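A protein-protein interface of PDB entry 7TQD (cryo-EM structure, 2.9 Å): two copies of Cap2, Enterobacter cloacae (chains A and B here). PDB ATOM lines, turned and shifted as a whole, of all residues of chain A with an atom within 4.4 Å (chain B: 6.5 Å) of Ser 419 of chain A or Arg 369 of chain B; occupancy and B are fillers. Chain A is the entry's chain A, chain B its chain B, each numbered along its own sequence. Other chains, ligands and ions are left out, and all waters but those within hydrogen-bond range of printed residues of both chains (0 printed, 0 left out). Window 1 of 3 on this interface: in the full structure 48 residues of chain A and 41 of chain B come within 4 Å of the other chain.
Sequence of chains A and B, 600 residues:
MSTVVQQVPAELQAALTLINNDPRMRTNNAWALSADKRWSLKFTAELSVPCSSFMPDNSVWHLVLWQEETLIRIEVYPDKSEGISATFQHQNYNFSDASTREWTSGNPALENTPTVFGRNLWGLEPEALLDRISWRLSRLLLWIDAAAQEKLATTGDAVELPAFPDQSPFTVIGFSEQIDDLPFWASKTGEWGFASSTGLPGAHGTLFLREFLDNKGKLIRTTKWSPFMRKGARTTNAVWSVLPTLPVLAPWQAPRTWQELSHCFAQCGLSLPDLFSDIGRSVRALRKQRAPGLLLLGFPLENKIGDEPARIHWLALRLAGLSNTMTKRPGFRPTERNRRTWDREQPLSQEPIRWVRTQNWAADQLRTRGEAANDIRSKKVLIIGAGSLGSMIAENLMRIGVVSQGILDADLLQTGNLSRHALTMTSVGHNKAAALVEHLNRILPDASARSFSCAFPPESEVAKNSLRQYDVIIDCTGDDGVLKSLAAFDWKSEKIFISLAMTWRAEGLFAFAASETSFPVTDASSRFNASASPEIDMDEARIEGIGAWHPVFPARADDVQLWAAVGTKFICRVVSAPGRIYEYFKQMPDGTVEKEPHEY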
ATOM      1  N   GLY A 416     -22.286  15.171  15.823  1.00  0.00           N
ATOM      2  CA  GLY A 416     -23.448  14.650  16.526  1.00  0.00           C
ATOM      3  C   GLY A 416     -23.778  15.432  17.783  1.00  0.00           C
ATOM      4  O   GLY A 416     -24.939  15.513  18.190  1.00  0.00           O
ATOM      5  N   ASN A 417     -22.759  16.012  18.421  1.00  0.00           N
ATOM      6  CA  ASN A 417     -22.976  16.738  19.667  1.00  0.00           C
ATOM      7  C   ASN A 417     -23.794  18.004  19.453  1.00  0.00           C
ATOM      8  O   ASN A 417     -24.399  18.517  20.400  1.00  0.00           O
ATOM      9  CB  ASN A 417     -21.636  17.085  20.313  1.00  0.00           C
ATOM     10  CG  ASN A 417     -20.787  15.865  20.577  1.00  0.00           C
ATOM     11  OD1 ASN A 417     -21.302  14.766  20.765  1.00  0.00           O
ATOM     12  ND2 ASN A 417     -19.474  16.053  20.592  1.00  0.00           N
ATOM     13  N   LEU A 418     -23.824  18.525  18.226  1.00  0.00           N
ATOM     14  CA  LEU A 418     -24.492  19.794  17.966  1.00  0.00           C
ATOM     15  C   LEU A 418     -26.007  19.703  18.062  1.00  0.00           C
ATOM     16  O   LEU A 418     -26.671  20.743  18.034  1.00  0.00           O
ATOM     17  CB  LEU A 418     -24.091  20.323  16.592  1.00  0.00           C
ATOM     18  CG  LEU A 418     -22.595  20.564  16.405  1.00  0.00           C
ATOM     19  CD1 LEU A 418     -22.302  20.970  14.980  1.00  0.00           C
ATOM     20  CD2 LEU A 418     -22.104  21.616  17.379  1.00  0.00           C
ATOM     21  N   SER A 419     -26.574  18.499  18.158  1.00  0.00           N
ATOM     22  CA  SER A 419     -28.017  18.388  18.339  1.00  0.00           C
ATOM     23  C   SER A 419     -28.447  18.962  19.682  1.00  0.00           C
ATOM     24  O   SER A 419     -29.571  19.455  19.824  1.00  0.00           O
ATOM     25  CB  SER A 419     -28.456  16.931  18.205  1.00  0.00           C
ATOM     26  OG  SER A 419     -27.966  16.138  19.269  1.00  0.00           O
ATOM     27  N   ARG A 420     -27.569  18.902  20.683  1.00  0.00           N
ATOM     28  CA  ARG A 420     -27.798  19.541  21.983  1.00  0.00           C
ATOM     29  C   ARG A 420     -26.483  20.179  22.429  1.00  0.00           C
ATOM     30  O   ARG A 420     -25.674  19.560  23.123  1.00  0.00           O
ATOM     31  CB  ARG A 420     -28.339  18.553  23.005  1.00  0.00           C
ATOM     32  CG  ARG A 420     -27.569  17.251  23.121  1.00  0.00           C
ATOM     33  CD  ARG A 420     -28.030  16.464  24.321  1.00  0.00           C
ATOM     34  NE  ARG A 420     -27.088  15.406  24.657  1.00  0.00           N
ATOM     35  CZ  ARG A 420     -27.258  14.132  24.335  1.00  0.00           C
ATOM     36  NH1 ARG A 420     -28.351  13.714  23.721  1.00  0.00           N
ATOM     37  NH2 ARG A 420     -26.319  13.250  24.658  1.00  0.00           N
ATOM     38  N   HIS A 421     -26.280  21.432  22.035  1.00  0.00           N
ATOM     39  CA  HIS A 421     -25.053  22.149  22.355  1.00  0.00           C
ATOM     40  C   HIS A 421     -25.278  23.629  22.090  1.00  0.00           C
ATOM     41  O   HIS A 421     -26.259  24.025  21.459  1.00  0.00           O
ATOM     42  CB  HIS A 421     -23.866  21.622  21.543  1.00  0.00           C
ATOM     43  CG  HIS A 421     -22.559  21.700  22.267  1.00  0.00           C
ATOM     44  ND1 HIS A 421     -21.704  22.772  22.144  1.00  0.00           N
ATOM     45  CD2 HIS A 421     -21.959  20.838  23.118  1.00  0.00           C
ATOM     46  CE1 HIS A 421     -20.636  22.571  22.893  1.00  0.00           C
ATOM     47  NE2 HIS A 421     -20.765  21.403  23.493  1.00  0.00           N
ATOM     48  N   VAL A 552     -26.444   6.105  23.145  1.00  0.00           N
ATOM     49  CA  VAL A 552     -26.373   7.453  23.695  1.00  0.00           C
ATOM     50  C   VAL A 552     -27.599   7.694  24.565  1.00  0.00           C
ATOM     51  O   VAL A 552     -28.606   6.990  24.469  1.00  0.00           O
ATOM     52  CB  VAL A 552     -26.276   8.528  22.594  1.00  0.00           C
ATOM     53  CG1 VAL A 552     -24.915   8.482  21.926  1.00  0.00           C
ATOM     54  CG2 VAL A 552     -27.378   8.334  21.571  1.00  0.00           C
ATOM     55  N   PHE A 553     -27.502   8.709  25.426  1.00  0.00           N
ATOM     56  CA  PHE A 553     -28.706   8.893  26.230  1.00  0.00           C
ATOM     57  C   PHE A 553     -29.633   9.918  25.579  1.00  0.00           C
ATOM     58  O   PHE A 553     -29.165  10.894  24.989  1.00  0.00           O
ATOM     59  CB  PHE A 553     -28.355   9.333  27.651  1.00  0.00           C
ATOM     60  CG  PHE A 553     -27.752  10.708  27.742  1.00  0.00           C
ATOM     61  CD1 PHE A 553     -26.392  10.895  27.576  1.00  0.00           C
ATOM     62  CD2 PHE A 553     -28.542  11.809  28.028  1.00  0.00           C
ATOM     63  CE1 PHE A 553     -25.838  12.156  27.671  1.00  0.00           C
ATOM     64  CE2 PHE A 553     -27.992  13.070  28.123  1.00  0.00           C
ATOM     65  CZ  PHE A 553     -26.639  13.243  27.944  1.00  0.00           C
ATOM     66  N   PRO A 554     -30.948   9.706  25.676  1.00  0.00           N
ATOM     67  CA  PRO A 554     -31.896  10.567  24.958  1.00  0.00           C
ATOM     68  C   PRO A 554     -32.138  11.876  25.696  1.00  0.00           C
ATOM     69  O   PRO A 554     -32.449  11.885  26.888  1.00  0.00           O
ATOM     70  CB  PRO A 554     -33.169   9.716  24.902  1.00  0.00           C
ATOM     71  CG  PRO A 554     -33.086   8.866  26.122  1.00  0.00           C
ATOM     72  CD  PRO A 554     -31.623   8.589  26.358  1.00  0.00           C
ATOM     73  N   ALA A 555     -32.001  12.985  24.971  1.00  0.00           N
ATOM     74  CA  ALA A 555     -32.291  14.307  25.510  1.00  0.00           C
ATOM     75  C   ALA A 555     -32.392  15.287  24.354  1.00  0.00           C
ATOM     76  O   ALA A 555     -31.497  15.338  23.507  1.00  0.00           O
ATOM     77  CB  ALA A 555     -31.214  14.756  26.501  1.00  0.00           C
ATOM     78  N   ALA A 557     -32.957  19.333  22.802  1.00  0.00           N
ATOM     79  CA  ALA A 557     -32.342  20.623  23.105  1.00  0.00           C
ATOM     80  C   ALA A 557     -33.174  21.427  24.099  1.00  0.00           C
ATOM     81  O   ALA A 557     -32.620  22.100  24.977  1.00  0.00           O
ATOM     82  CB  ALA A 557     -32.132  21.417  21.820  1.00  0.00           C
ATOM     83  N   GLN B 365     -28.791  10.262  10.359  1.00  0.00           N
ATOM     84  CA  GLN B 365     -27.616   9.954  11.162  1.00  0.00           C
ATOM     85  C   GLN B 365     -27.114  11.150  11.957  1.00  0.00           C
ATOM     86  O   GLN B 365     -26.085  11.043  12.632  1.00  0.00           O
ATOM     87  CB  GLN B 365     -26.494   9.416  10.271  1.00  0.00           C
ATOM     88  CG  GLN B 365     -26.868   8.181   9.480  1.00  0.00           C
ATOM     89  CD  GLN B 365     -26.814   6.928  10.320  1.00  0.00           C
ATOM     90  OE1 GLN B 365     -25.950   6.785  11.183  1.00  0.00           O
ATOM     91  NE2 GLN B 365     -27.738   6.010  10.075  1.00  0.00           N
ATOM     92  N   LEU B 366     -27.804  12.285  11.895  1.00  0.00           N
ATOM     93  CA  LEU B 366     -27.345  13.489  12.575  1.00  0.00           C
ATOM     94  C   LEU B 366     -27.949  13.673  13.957  1.00  0.00           C
ATOM     95  O   LEU B 366     -27.286  14.225  14.840  1.00  0.00           O
ATOM     96  CB  LEU B 366     -27.653  14.730  11.731  1.00  0.00           C
ATOM     97  CG  LEU B 366     -26.710  15.024  10.565  1.00  0.00           C
ATOM     98  CD1 LEU B 366     -27.276  16.122   9.690  1.00  0.00           C
ATOM     99  CD2 LEU B 366     -25.332  15.403  11.073  1.00  0.00           C
ATOM    100  N   ARG B 367     -29.183  13.226  14.175  1.00  0.00           N
ATOM    101  CA  ARG B 367     -29.856  13.474  15.443  1.00  0.00           C
ATOM    102  C   ARG B 367     -30.255  12.176  16.129  1.00  0.00           C
ATOM    103  O   ARG B 367     -31.390  12.037  16.591  1.00  0.00           O
ATOM    104  CB  ARG B 367     -31.081  14.363  15.228  1.00  0.00           C
ATOM    105  CG  ARG B 367     -30.747  15.727  14.651  1.00  0.00           C
ATOM    106  CD  ARG B 367     -31.999  16.482  14.256  1.00  0.00           C
ATOM    107  NE  ARG B 367     -31.690  17.744  13.597  1.00  0.00           N
ATOM    108  CZ  ARG B 367     -31.541  17.888  12.288  1.00  0.00           C
ATOM    109  NH1 ARG B 367     -31.647  16.860  11.465  1.00  0.00           N
ATOM    110  NH2 ARG B 367     -31.283  19.094  11.792  1.00  0.00           N
ATOM    111  N   THR B 368     -29.332  11.218  16.200  1.00  0.00           N
ATOM    112  CA  THR B 368     -29.584   9.972  16.915  1.00  0.00           C
ATOM    113  C   THR B 368     -29.664  10.166  18.421  1.00  0.00           C
ATOM    114  O   THR B 368     -30.044   9.228  19.128  1.00  0.00           O
ATOM    115  CB  THR B 368     -28.501   8.943  16.585  1.00  0.00           C
ATOM    116  OG1 THR B 368     -27.214   9.483  16.907  1.00  0.00           O
ATOM    117  CG2 THR B 368     -28.538   8.582  15.110  1.00  0.00           C
ATOM    118  N   ARG B 369     -29.320  11.351  18.923  1.00  0.00           N
ATOM    119  CA  ARG B 369     -29.343  11.653  20.346  1.00  0.00           C
ATOM    120  C   ARG B 369     -30.666  12.257  20.804  1.00  0.00           C
ATOM    121  O   ARG B 369     -30.790  12.629  21.974  1.00  0.00           O
ATOM    122  CB  ARG B 369     -28.194  12.601  20.694  1.00  0.00           C
ATOM    123  CG  ARG B 369     -26.810  12.023  20.462  1.00  0.00           C
ATOM    124  CD  ARG B 369     -25.771  13.126  20.346  1.00  0.00           C
ATOM    125  NE  ARG B 369     -24.417  12.623  20.543  1.00  0.00           N
ATOM    126  CZ  ARG B 369     -23.676  12.074  19.592  1.00  0.00           C
ATOM    127  NH1 ARG B 369     -24.130  11.932  18.357  1.00  0.00           N
ATOM    128  NH2 ARG B 369     -22.450  11.654  19.886  1.00  0.00           N
ATOM    129  N   GLY B 370     -31.651  12.367  19.916  1.00  0.00           N
ATOM    130  CA  GLY B 370     -32.934  12.943  20.268  1.00  0.00           C
ATOM    131  C   GLY B 370     -33.470  13.909  19.229  1.00  0.00           C
ATOM    132  O   GLY B 370     -32.791  14.870  18.857  1.00  0.00           O
ATOM    133  N   GLU B 371     -34.696  13.671  18.764  1.00  0.00           N
ATOM    134  CA  GLU B 371     -35.283  14.471  17.699  1.00  0.00           C
ATOM    135  C   GLU B 371     -36.791  14.534  17.890  1.00  0.00           C
ATOM    136  O   GLU B 371     -37.378  13.740  18.629  1.00  0.00           O
ATOM    137  CB  GLU B 371     -34.952  13.897  16.318  1.00  0.00           C
ATOM    138  CG  GLU B 371     -35.377  12.448  16.142  1.00  0.00           C
ATOM    139  CD  GLU B 371     -34.765  11.795  14.919  1.00  0.00           C
ATOM    140  OE1 GLU B 371     -33.945  12.445  14.238  1.00  0.00           O
ATOM    141  OE2 GLU B 371     -35.108  10.628  14.638  1.00  0.00           O
ATOM    142  N   ARG B 399     -32.454  22.861  15.793  1.00  0.00           N
ATOM    143  CA  ARG B 399     -31.681  21.796  16.423  1.00  0.00           C
ATOM    144  C   ARG B 399     -32.497  20.533  16.667  1.00  0.00           C
ATOM    145  O   ARG B 399     -31.912  19.450  16.756  1.00  0.00           O
ATOM    146  CB  ARG B 399     -31.072  22.281  17.738  1.00  0.00           C
ATOM    147  CG  ARG B 399     -29.888  23.211  17.561  1.00  0.00           C
ATOM    148  CD  ARG B 399     -29.068  23.324  18.832  1.00  0.00           C
ATOM    149  NE  ARG B 399     -28.240  24.523  18.835  1.00  0.00           N
ATOM    150  CZ  ARG B 399     -26.976  24.557  18.440  1.00  0.00           C
ATOM    151  NH1 ARG B 399     -26.355  23.469  18.022  1.00  0.00           N
ATOM    152  NH2 ARG B 399     -26.320  25.711  18.463  1.00  0.00           N
ATOM    153  N   ILE B 400     -33.824  20.630  16.781  1.00  0.00           N
ATOM    154  CA  ILE B 400     -34.627  19.440  17.069  1.00  0.00           C
ATOM    155  C   ILE B 400     -35.180  18.759  15.823  1.00  0.00           C
ATOM    156  O   ILE B 400     -35.785  17.681  15.946  1.00  0.00           O
ATOM    157  CB  ILE B 400     -35.789  19.748  18.038  1.00  0.00           C
ATOM    158  CG1 ILE B 400     -36.793  20.705  17.397  1.00  0.00           C
ATOM    159  CG2 ILE B 400     -35.262  20.280  19.358  1.00  0.00           C
ATOM    160  CD1 ILE B 400     -38.029  20.920  18.226  1.00  0.00           C
ATOM    161  N   LEU B 444     -26.299  22.830  11.289  1.00  0.00           N
ATOM    162  CA  LEU B 444     -26.215  21.436  10.887  1.00  0.00           C
ATOM    163  C   LEU B 444     -26.198  21.339   9.370  1.00  0.00           C
ATOM    164  O   LEU B 444     -26.639  22.262   8.677  1.00  0.00           O
ATOM    165  CB  LEU B 444     -27.391  20.633  11.462  1.00  0.00           C
ATOM    166  CG  LEU B 444     -27.212  20.189  12.915  1.00  0.00           C
ATOM    167  CD1 LEU B 444     -28.481  19.570  13.460  1.00  0.00           C
ATOM    168  CD2 LEU B 444     -26.053  19.220  13.046  1.00  0.00           C
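Arg 369 of chain B touches Gly 416 of chain A. Ser 419 of chain A touches Arg 369 of chain B. Ser 419 of chain A touches Arg 399 of chain B. O of Thr 368 of chain B touches CG2 of Val 552 of chain A (3.7 Å). Arg 369 of chain B touches Val 552 of chain A (CG to CG2, 3.9 Å). Arg 369 of chain B touches Phe 553 of chain A. O of Arg 369 of chain B touches CA of Pro 554 of chain A, at 3.8 Å.
No position is printed for both chains.
Of the 10 printed residues of chain B, 3 touch a printed residue of chain A. Printed residues of chain A that touch a printed residue of chain B: Gly 416, Asn 417, Leu 418, Ser 419, Arg 420, His 421, Val 552, Phe 553, Pro 554 and Ala 555. Hydrophobic or aromatic side chains of chain A within 4 Å of the printed part of chain B: Val 552.
OG of Ser 419 of chain A sits at hydrogen-bond distance from O of Gly 416 of chain A, at 3.3 Å. O of Phe 553 of chain A lies within hydrogen-bond range of NH1 of Arg 420 of chain A (3.2 Å).
The side-chain amide oxygen of Asn 417 of chain A is in hydrogen-bond range of the guanidinium group of Arg 369 of chain B. NH1 of Arg 399 of chain B sits at hydrogen-bond distance from O of Leu 418 of chain A (2.7 Å). NH1 of Arg 420 of chain A lies within hydrogen-bond range of O of Arg 369 of chain B (3.2 Å). The guanidinium group (NE) of Arg 399 of chain B lies close to the backbone carbonyl oxygen (O) of His 421 of chain A. The backbone NH (N) of Ala 555 of chain A sits at hydrogen-bond distance from the backbone carbonyl oxygen (O) of Arg 369 of chain B, at 3.3 Å.
Arg 369 of chain B touches eight residues of chain A. Printed residues of chain B within 4 Å of Leu 418 of chain A: Arg 399. Of the printed residues of chain B, Val 552 of chain A touches Thr 368 (3.7 Å) and Arg 369 (3.9 Å). Of the printed residues of chain B, Gly 416 of chain A touches Arg 369 (3.3 Å). Of the printed residues of chain B, Arg 420 of chain A touches Arg 369. Arg 367 of chain B touches none of the printed residues of chain A. Leu 366 of chain B touches none of the printed residues of chain A. The nearest printed residue of chain A that does not touch Arg 369 of chain B is Leu 418 of chain A (6.1 Å). The nearest printed residue of chain B that does not touch Leu 418 of chain A is Leu 444 of chain B (4.2 Å).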
